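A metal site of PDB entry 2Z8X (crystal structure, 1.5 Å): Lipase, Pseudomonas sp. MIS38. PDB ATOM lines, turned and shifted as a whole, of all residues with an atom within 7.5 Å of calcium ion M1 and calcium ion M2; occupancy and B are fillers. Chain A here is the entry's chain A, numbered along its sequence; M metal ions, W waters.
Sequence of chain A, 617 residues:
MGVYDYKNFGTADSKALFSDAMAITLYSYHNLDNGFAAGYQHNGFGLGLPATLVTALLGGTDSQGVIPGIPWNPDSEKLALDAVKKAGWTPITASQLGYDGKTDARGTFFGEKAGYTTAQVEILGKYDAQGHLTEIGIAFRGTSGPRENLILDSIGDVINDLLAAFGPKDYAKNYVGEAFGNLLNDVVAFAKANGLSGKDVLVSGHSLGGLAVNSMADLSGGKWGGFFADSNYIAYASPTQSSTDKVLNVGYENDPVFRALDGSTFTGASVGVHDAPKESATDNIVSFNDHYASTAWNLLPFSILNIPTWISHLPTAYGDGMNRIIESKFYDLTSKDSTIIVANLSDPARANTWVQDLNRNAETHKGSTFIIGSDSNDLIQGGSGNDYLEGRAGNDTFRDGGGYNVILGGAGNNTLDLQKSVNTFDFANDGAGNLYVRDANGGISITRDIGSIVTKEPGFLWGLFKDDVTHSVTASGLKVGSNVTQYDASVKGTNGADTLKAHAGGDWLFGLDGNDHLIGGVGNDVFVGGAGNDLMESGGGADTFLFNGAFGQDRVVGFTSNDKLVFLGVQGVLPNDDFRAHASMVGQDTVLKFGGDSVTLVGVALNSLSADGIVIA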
ATOM      1  N   ASN A 249     -22.232 -17.585   0.559  1.00  0.00           N
ATOM      2  CA  ASN A 249     -21.538 -18.589   1.371  1.00  0.00           C
ATOM      3  C   ASN A 249     -20.111 -18.120   1.668  1.00  0.00           C
ATOM      4  O   ASN A 249     -19.239 -18.172   0.795  1.00  0.00           O
ATOM      5  CB  ASN A 249     -21.541 -19.962   0.682  1.00  0.00           C
ATOM      6  CG  ASN A 249     -22.828 -20.740   0.914  1.00  0.00           C
ATOM      7  OD1 ASN A 249     -23.566 -21.076  -0.036  1.00  0.00           O
ATOM      8  ND2 ASN A 249     -23.135 -21.009   2.171  1.00  0.00           N
ATOM      9  N   GLU A 253     -10.836 -20.485   3.430  1.00  0.00           N
ATOM     10  CA  GLU A 253     -10.378 -21.510   2.507  1.00  0.00           C
ATOM     11  C   GLU A 253      -9.845 -22.735   3.232  1.00  0.00           C
ATOM     12  O   GLU A 253     -10.044 -23.867   2.787  1.00  0.00           O
ATOM     13  CB  GLU A 253      -9.288 -20.866   1.644  1.00  0.00           C
ATOM     14  CG  GLU A 253      -8.558 -21.753   0.704  1.00  0.00           C
ATOM     15  CD  GLU A 253      -7.533 -20.972  -0.082  1.00  0.00           C
ATOM     16  OE1 GLU A 253      -6.435 -20.726   0.443  1.00  0.00           O
ATOM     17  OE2 GLU A 253      -7.831 -20.603  -1.233  1.00  0.00           O
ATOM     18  N   ASN A 254      -9.155 -22.486   4.355  1.00  0.00           N
ATOM     19  CA  ASN A 254      -8.549 -23.555   5.135  1.00  0.00           C
ATOM     20  C   ASN A 254      -9.445 -24.113   6.235  1.00  0.00           C
ATOM     21  O   ASN A 254      -9.003 -24.930   7.053  1.00  0.00           O
ATOM     22  CB  ASN A 254      -7.150 -23.152   5.652  1.00  0.00           C
ATOM     23  CG  ASN A 254      -7.141 -21.832   6.390  1.00  0.00           C
ATOM     24  OD1 ASN A 254      -7.835 -20.882   6.027  1.00  0.00           O
ATOM     25  ND2 ASN A 254      -6.314 -21.752   7.435  1.00  0.00           N
ATOM     26  N   ARG A 259     -17.514 -25.743   2.426  1.00  0.00           N
ATOM     27  CA  ARG A 259     -17.571 -26.317   1.067  1.00  0.00           C
ATOM     28  C   ARG A 259     -17.163 -27.795   1.011  1.00  0.00           C
ATOM     29  O   ARG A 259     -16.753 -28.284  -0.060  1.00  0.00           O
ATOM     30  CB  ARG A 259     -16.705 -25.520   0.092  1.00  0.00           C
ATOM     31  CG  ARG A 259     -16.918 -24.001   0.075  1.00  0.00           C
ATOM     32  CD  ARG A 259     -15.796 -23.328  -0.702  1.00  0.00           C
ATOM     33  NE  ARG A 259     -14.501 -23.612  -0.069  1.00  0.00           N
ATOM     34  CZ  ARG A 259     -13.312 -23.403  -0.642  1.00  0.00           C
ATOM     35  NH1 ARG A 259     -13.220 -22.884  -1.859  1.00  0.00           N
ATOM     36  NH2 ARG A 259     -12.213 -23.741   0.031  1.00  0.00           N
ATOM     37  N   HIS A 274     -10.868 -29.450  -0.599  1.00  0.00           N
ATOM     38  CA  HIS A 274     -12.047 -29.248  -1.455  1.00  0.00           C
ATOM     39  C   HIS A 274     -12.199 -27.770  -1.783  1.00  0.00           C
ATOM     40  O   HIS A 274     -13.145 -27.099  -1.347  1.00  0.00           O
ATOM     41  CB  HIS A 274     -13.320 -29.824  -0.807  1.00  0.00           C
ATOM     42  CG  HIS A 274     -13.386 -29.609   0.671  1.00  0.00           C
ATOM     43  ND1 HIS A 274     -13.699 -28.390   1.230  1.00  0.00           N
ATOM     44  CD2 HIS A 274     -13.175 -30.454   1.711  1.00  0.00           C
ATOM     45  CE1 HIS A 274     -13.692 -28.498   2.550  1.00  0.00           C
ATOM     46  NE2 HIS A 274     -13.374 -29.741   2.869  1.00  0.00           N
ATOM     47  N   ASP A 275     -11.267 -27.288  -2.605  1.00  0.00           N
ATOM     48  CA  ASP A 275     -11.113 -25.867  -2.861  1.00  0.00           C
ATOM     49  C   ASP A 275     -11.473 -25.485  -4.304  1.00  0.00           C
ATOM     50  O   ASP A 275     -10.992 -24.463  -4.807  1.00  0.00           O
ATOM     51  CB  ASP A 275      -9.672 -25.449  -2.538  1.00  0.00           C
ATOM     52  CG  ASP A 275      -9.484 -23.943  -2.568  1.00  0.00           C
ATOM     53  OD1 ASP A 275     -10.374 -23.189  -2.109  1.00  0.00           O
ATOM     54  OD2 ASP A 275      -8.427 -23.505  -3.062  1.00  0.00           O
ATOM     55  N   ALA A 276     -12.302 -26.283  -4.966  1.00  0.00           N
ATOM     56  CA  ALA A 276     -12.746 -25.924  -6.299  1.00  0.00           C
ATOM     57  C   ALA A 276     -13.650 -24.684  -6.211  1.00  0.00           C
ATOM     58  O   ALA A 276     -14.444 -24.564  -5.289  1.00  0.00           O
ATOM     59  CB  ALA A 276     -13.502 -27.089  -6.933  1.00  0.00           C
ATOM     60  N   PRO A 277     -13.513 -23.762  -7.184  1.00  0.00           N
ATOM     61  CA  PRO A 277     -14.365 -22.573  -7.142  1.00  0.00           C
ATOM     62  C   PRO A 277     -15.868 -22.901  -7.100  1.00  0.00           C
ATOM     63  O   PRO A 277     -16.327 -23.854  -7.756  1.00  0.00           O
ATOM     64  CB  PRO A 277     -14.009 -21.844  -8.438  1.00  0.00           C
ATOM     65  CG  PRO A 277     -12.599 -22.266  -8.698  1.00  0.00           C
ATOM     66  CD  PRO A 277     -12.577 -23.711  -8.317  1.00  0.00           C
ATOM     67  N   LYS A 278     -16.607 -22.122  -6.331  1.00  0.00           N
ATOM     68  CA  LYS A 278     -18.060 -22.253  -6.243  1.00  0.00           C
ATOM     69  C   LYS A 278     -18.709 -20.889  -6.379  1.00  0.00           C
ATOM     70  O   LYS A 278     -18.282 -19.919  -5.734  1.00  0.00           O
ATOM     71  CB  LYS A 278     -18.449 -22.920  -4.917  1.00  0.00           C
ATOM     72  CG  LYS A 278     -18.107 -24.413  -4.896  1.00  0.00           C
ATOM     73  CD  LYS A 278     -18.386 -25.080  -3.544  1.00  0.00           C
ATOM     74  CE  LYS A 278     -18.388 -26.612  -3.672  1.00  0.00           C
ATOM     75  NZ  LYS A 278     -17.095 -27.110  -4.216  1.00  0.00           N
ATOM     76  N   GLU A 279     -19.739 -20.810  -7.217  1.00  0.00           N
ATOM     77  CA  GLU A 279     -20.360 -19.543  -7.556  1.00  0.00           C
ATOM     78  C   GLU A 279     -20.880 -18.783  -6.322  1.00  0.00           C
ATOM     79  O   GLU A 279     -20.759 -17.571  -6.222  1.00  0.00           O
ATOM     80  CB  GLU A 279     -21.469 -19.762  -8.582  1.00  0.00           C
ATOM     81  CG  GLU A 279     -22.089 -18.494  -9.133  1.00  0.00           C
ATOM     82  CD  GLU A 279     -23.232 -17.956  -8.281  1.00  0.00           C
ATOM     83  OE1 GLU A 279     -23.826 -18.738  -7.505  1.00  0.00           O
ATOM     84  OE2 GLU A 279     -23.541 -16.740  -8.405  1.00  0.00           O
ATOM     85  N   SER A 280     -21.481 -19.513  -5.383  1.00  0.00           N
ATOM     86  CA  SER A 280     -22.069 -18.841  -4.221  1.00  0.00           C
ATOM     87  C   SER A 280     -21.038 -18.463  -3.151  1.00  0.00           C
ATOM     88  O   SER A 280     -21.369 -17.714  -2.231  1.00  0.00           O
ATOM     89  CB  SER A 280     -23.143 -19.724  -3.577  1.00  0.00           C
ATOM     90  OG  SER A 280     -22.559 -20.841  -2.931  1.00  0.00           O
ATOM     91  N   ALA A 281     -19.819 -18.971  -3.284  1.00  0.00           N
ATOM     92  CA  ALA A 281     -18.866 -18.939  -2.173  1.00  0.00           C
ATOM     93  C   ALA A 281     -17.668 -18.001  -2.382  1.00  0.00           C
ATOM     94  O   ALA A 281     -17.190 -17.828  -3.512  1.00  0.00           O
ATOM     95  CB  ALA A 281     -18.349 -20.337  -1.894  1.00  0.00           C
ATOM     96  N   THR A 282     -17.188 -17.443  -1.277  1.00  0.00           N
ATOM     97  CA  THR A 282     -15.896 -16.742  -1.250  1.00  0.00           C
ATOM     98  C   THR A 282     -14.816 -17.806  -1.174  1.00  0.00           C
ATOM     99  O   THR A 282     -14.675 -18.479  -0.151  1.00  0.00           O
ATOM    100  CB  THR A 282     -15.782 -15.839   0.000  1.00  0.00           C
ATOM    101  OG1 THR A 282     -16.020 -16.615   1.188  1.00  0.00           O
ATOM    102  CG2 THR A 282     -16.787 -14.686  -0.062  1.00  0.00           C
ATOM    103  N   ASP A 283     -14.045 -17.969  -2.237  1.00  0.00           N
ATOM    104  CA  ASP A 283     -13.175 -19.142  -2.341  1.00  0.00           C
ATOM    105  C   ASP A 283     -11.732 -19.005  -1.885  1.00  0.00           C
ATOM    106  O   ASP A 283     -11.016 -20.015  -1.806  1.00  0.00           O
ATOM    107  CB  ASP A 283     -13.245 -19.722  -3.750  1.00  0.00           C
ATOM    108  CG  ASP A 283     -14.591 -20.358  -4.038  1.00  0.00           C
ATOM    109  OD1 ASP A 283     -15.049 -21.223  -3.252  1.00  0.00           O
ATOM    110  OD2 ASP A 283     -15.193 -20.012  -5.073  1.00  0.00           O
ATOM    111  N   ASN A 284     -11.282 -17.804  -1.558  1.00  0.00           N
ATOM    112  CA  ASN A 284      -9.854 -17.569  -1.357  1.00  0.00           C
ATOM    113  C   ASN A 284      -9.492 -16.670  -0.163  1.00  0.00           C
ATOM    114  O   ASN A 284      -8.549 -15.890  -0.227  1.00  0.00           O
ATOM    115  CB  ASN A 284      -9.215 -17.018  -2.632  1.00  0.00           C
ATOM    116  CG  ASN A 284      -9.487 -17.921  -3.835  1.00  0.00           C
ATOM    117  OD1 ASN A 284      -9.069 -19.046  -3.852  1.00  0.00           O
ATOM    118  ND2 ASN A 284     -10.179 -17.395  -4.824  1.00  0.00           N
ATOM    119  N   ILE A 285     -10.277 -16.778   0.900  1.00  0.00           N
ATOM    120  CA  ILE A 285      -9.981 -16.062   2.140  1.00  0.00           C
ATOM    121  C   ILE A 285      -9.266 -17.010   3.091  1.00  0.00           C
ATOM    122  O   ILE A 285      -9.850 -18.000   3.539  1.00  0.00           O
ATOM    123  CB  ILE A 285     -11.253 -15.491   2.834  1.00  0.00           C
ATOM    124  CG1 ILE A 285     -12.102 -14.674   1.859  1.00  0.00           C
ATOM    125  CG2 ILE A 285     -10.857 -14.639   4.031  1.00  0.00           C
ATOM    126  CD1 ILE A 285     -13.442 -14.200   2.439  1.00  0.00           C
ATOM    127  N   VAL A 286      -7.999 -16.720   3.384  1.00  0.00           N
ATOM    128  CA  VAL A 286      -7.171 -17.598   4.229  1.00  0.00           C
ATOM    129  C   VAL A 286      -7.135 -17.108   5.667  1.00  0.00           C
ATOM    130  O   VAL A 286      -6.906 -15.922   5.931  1.00  0.00           O
ATOM    131  CB  VAL A 286      -5.715 -17.655   3.684  1.00  0.00           C
ATOM    132  CG1 VAL A 286      -4.779 -18.440   4.613  1.00  0.00           C
ATOM    133  CG2 VAL A 286      -5.703 -18.241   2.289  1.00  0.00           C
ATOM    134  N   LYS A 336     -15.598 -11.132  -4.709  1.00  0.00           N
ATOM    135  CA  LYS A 336     -15.997 -12.364  -4.011  1.00  0.00           C
ATOM    136  C   LYS A 336     -14.869 -13.380  -3.897  1.00  0.00           C
ATOM    137  O   LYS A 336     -14.699 -14.013  -2.841  1.00  0.00           O
ATOM    138  CB  LYS A 336     -17.201 -12.984  -4.736  1.00  0.00           C
ATOM    139  CG  LYS A 336     -17.939 -14.040  -3.964  1.00  0.00           C
ATOM    140  CD  LYS A 336     -19.318 -14.181  -4.581  1.00  0.00           C
ATOM    141  CE  LYS A 336     -20.109 -15.277  -3.935  1.00  0.00           C
ATOM    142  NZ  LYS A 336     -21.547 -15.102  -4.307  1.00  0.00           N
ATOM    143  N   ASP A 337     -14.079 -13.519  -4.959  1.00  0.00           N
ATOM    144  CA  ASP A 337     -13.007 -14.521  -4.985  1.00  0.00           C
ATOM    145  C   ASP A 337     -11.586 -13.924  -4.915  1.00  0.00           C
ATOM    146  O   ASP A 337     -10.617 -14.588  -5.267  1.00  0.00           O
ATOM    147  CB  ASP A 337     -13.175 -15.477  -6.171  1.00  0.00           C
ATOM    148  CG  ASP A 337     -14.376 -16.388  -6.004  1.00  0.00           C
ATOM    149  OD1 ASP A 337     -14.636 -16.825  -4.853  1.00  0.00           O
ATOM    150  OD2 ASP A 337     -15.090 -16.668  -7.003  1.00  0.00           O
ATOM    151  N   THR A 339      -8.080 -13.033  -3.329  1.00  0.00           N
ATOM    152  CA  THR A 339      -7.221 -13.707  -2.374  1.00  0.00           C
ATOM    153  C   THR A 339      -6.982 -12.764  -1.202  1.00  0.00           C
ATOM    154  O   THR A 339      -6.360 -11.710  -1.367  1.00  0.00           O
ATOM    155  CB  THR A 339      -5.862 -14.023  -3.000  1.00  0.00           C
ATOM    156  OG1 THR A 339      -6.056 -14.743  -4.226  1.00  0.00           O
ATOM    157  CG2 THR A 339      -4.993 -14.838  -2.026  1.00  0.00           C
ATOM    158  N   ASN A 359      -0.230 -20.396   0.164  1.00  0.00           N
ATOM    159  CA  ASN A 359      -1.033 -21.156  -0.805  1.00  0.00           C
ATOM    160  C   ASN A 359      -1.129 -22.639  -0.426  1.00  0.00           C
ATOM    161  O   ASN A 359      -1.271 -23.496  -1.294  1.00  0.00           O
ATOM    162  CB  ASN A 359      -0.486 -21.006  -2.236  1.00  0.00           C
ATOM    163  CG  ASN A 359      -1.603 -20.957  -3.297  1.00  0.00           C
ATOM    164  OD1 ASN A 359      -1.599 -20.084  -4.161  1.00  0.00           O
ATOM    165  ND2 ASN A 359      -2.556 -21.887  -3.219  1.00  0.00           N
ATOM    166  N   ASN A 361      -2.685 -26.088   0.844  1.00  0.00           N
ATOM    167  CA  ASN A 361      -3.976 -26.803   0.820  1.00  0.00           C
ATOM    168  C   ASN A 361      -5.064 -26.035   0.081  1.00  0.00           C
ATOM    169  O   ASN A 361      -6.189 -25.854   0.559  1.00  0.00           O
ATOM    170  CB  ASN A 361      -4.424 -27.105   2.256  1.00  0.00           C
ATOM    171  CG  ASN A 361      -3.507 -28.055   2.956  1.00  0.00           C
ATOM    172  OD1 ASN A 361      -3.031 -29.012   2.344  1.00  0.00           O
ATOM    173  ND2 ASN A 361      -3.243 -27.807   4.228  1.00  0.00           N
ATOM    174  N   ALA A 362      -4.707 -25.579  -1.113  1.00  0.00           N
ATOM    175  CA  ALA A 362      -5.580 -24.736  -1.905  1.00  0.00           C
ATOM    176  C   ALA A 362      -5.135 -24.743  -3.354  1.00  0.00           C
ATOM    177  O   ALA A 362      -3.951 -24.941  -3.648  1.00  0.00           O
ATOM    178  CB  ALA A 362      -5.566 -23.309  -1.359  1.00  0.00           C
ATOM    179  N   GLU A 363      -6.077 -24.488  -4.243  1.00  0.00           N
ATOM    180  CA  GLU A 363      -5.762 -24.291  -5.651  1.00  0.00           C
ATOM    181  C   GLU A 363      -4.902 -23.024  -5.785  1.00  0.00           C
ATOM    182  O   GLU A 363      -4.931 -22.155  -4.909  1.00  0.00           O
ATOM    183  CB  GLU A 363      -7.050 -24.250  -6.480  1.00  0.00           C
ATOM    184  CG  GLU A 363      -7.864 -25.546  -6.238  1.00  0.00           C
ATOM    185  CD  GLU A 363      -8.957 -25.859  -7.264  1.00  0.00           C
ATOM    186  OE1 GLU A 363      -9.212 -25.046  -8.180  1.00  0.00           O
ATOM    187  OE2 GLU A 363      -9.578 -26.941  -7.128  1.00  0.00           O
ATOM    188  N   THR A 364      -4.116 -22.933  -6.859  1.00  0.00           N
ATOM    189  CA  THR A 364      -3.230 -21.792  -7.037  1.00  0.00           C
ATOM    190  C   THR A 364      -4.001 -20.483  -7.033  1.00  0.00           C
ATOM    191  O   THR A 364      -4.991 -20.334  -7.772  1.00  0.00           O
ATOM    192  CB  THR A 364      -2.399 -21.939  -8.331  1.00  0.00           C
ATOM    193  OG1 THR A 364      -1.680 -23.180  -8.276  1.00  0.00           O
ATOM    194  CG2 THR A 364      -1.412 -20.785  -8.485  1.00  0.00           C
ATOM    195  N   HIS A 365      -3.574 -19.553  -6.190  1.00  0.00           N
ATOM    196  CA  HIS A 365      -4.231 -18.245  -6.101  1.00  0.00           C
ATOM    197  C   HIS A 365      -3.949 -17.412  -7.340  1.00  0.00           C
ATOM    198  O   HIS A 365      -2.844 -17.461  -7.901  1.00  0.00           O
ATOM    199  CB  HIS A 365      -3.817 -17.501  -4.842  1.00  0.00           C
ATOM    200  CG  HIS A 365      -4.332 -18.128  -3.589  1.00  0.00           C
ATOM    201  ND1 HIS A 365      -3.614 -18.147  -2.409  1.00  0.00           N
ATOM    202  CD2 HIS A 365      -5.507 -18.751  -3.317  1.00  0.00           C
ATOM    203  CE1 HIS A 365      -4.322 -18.770  -1.479  1.00  0.00           C
ATOM    204  NE2 HIS A 365      -5.473 -19.144  -2.009  1.00  0.00           N
HETATM  205 CA    CA M   1     -16.531 -18.229  -5.759  1.00  0.00          CA
HETATM  206 CA    CA M   2      -9.205 -21.174  -2.925  1.00  0.00          CA
HETATM  207  O   HOH W   1     -16.411 -19.158  -8.019  1.00  0.00           O
HETATM  208  O   HOH W   2     -18.149 -16.681  -6.556  1.00  0.00           O
HETATM  209  O   HOH W   3     -10.634 -21.772  -4.805  1.00  0.00           O
HETATM  210  O   HOH W   4      -7.395 -21.045  -4.417  1.00  0.00           O
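Calcium ion M2 is bound by the side-chain carboxylate (OE2) of Glu 253, the side-chain amide oxygen (OD1) of Asn 284, water W4, the backbone carbonyl oxygen (O) of Asp 283, water W3, the side-chain carboxylate (OD2) of Asp 275 and the side-chain carboxylate (OD1) of Asp 275.
Calcium ion M2 has seven donor atoms within binding distance.
The nearest printed residue that does not touch calcium ion M1 is Glu 279 (4.3 Å).
NE2 of His 365 sits at hydrogen-bond distance from OE1 of Glu 253, at 3.1 Å.
ND2 of Asn 284 lies within hydrogen-bond range of O of Asp 337, at 2.9 Å.
The guanidinium group of Arg 259 sits close to the side-chain carboxylate of Asp 275, 2.9 Å away.
The guanidinium group of Arg 259 lies within salt-bridge range of the side-chain carboxylate of Asp 283 (2.8 Å).
The backbone NH of Glu 363 sits close to the side-chain carboxylate of Asp 275 (2.8 Å).
N of Glu 253 is in hydrogen-bond range of O of Ile 285 (2.7 Å).
Calcium ion M1 is bound by OD2 of Asp 283, O of Ala 281, water W2, O of Lys 278, water W1, OD2 of Asp 337 and OD1 of Asp 337.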
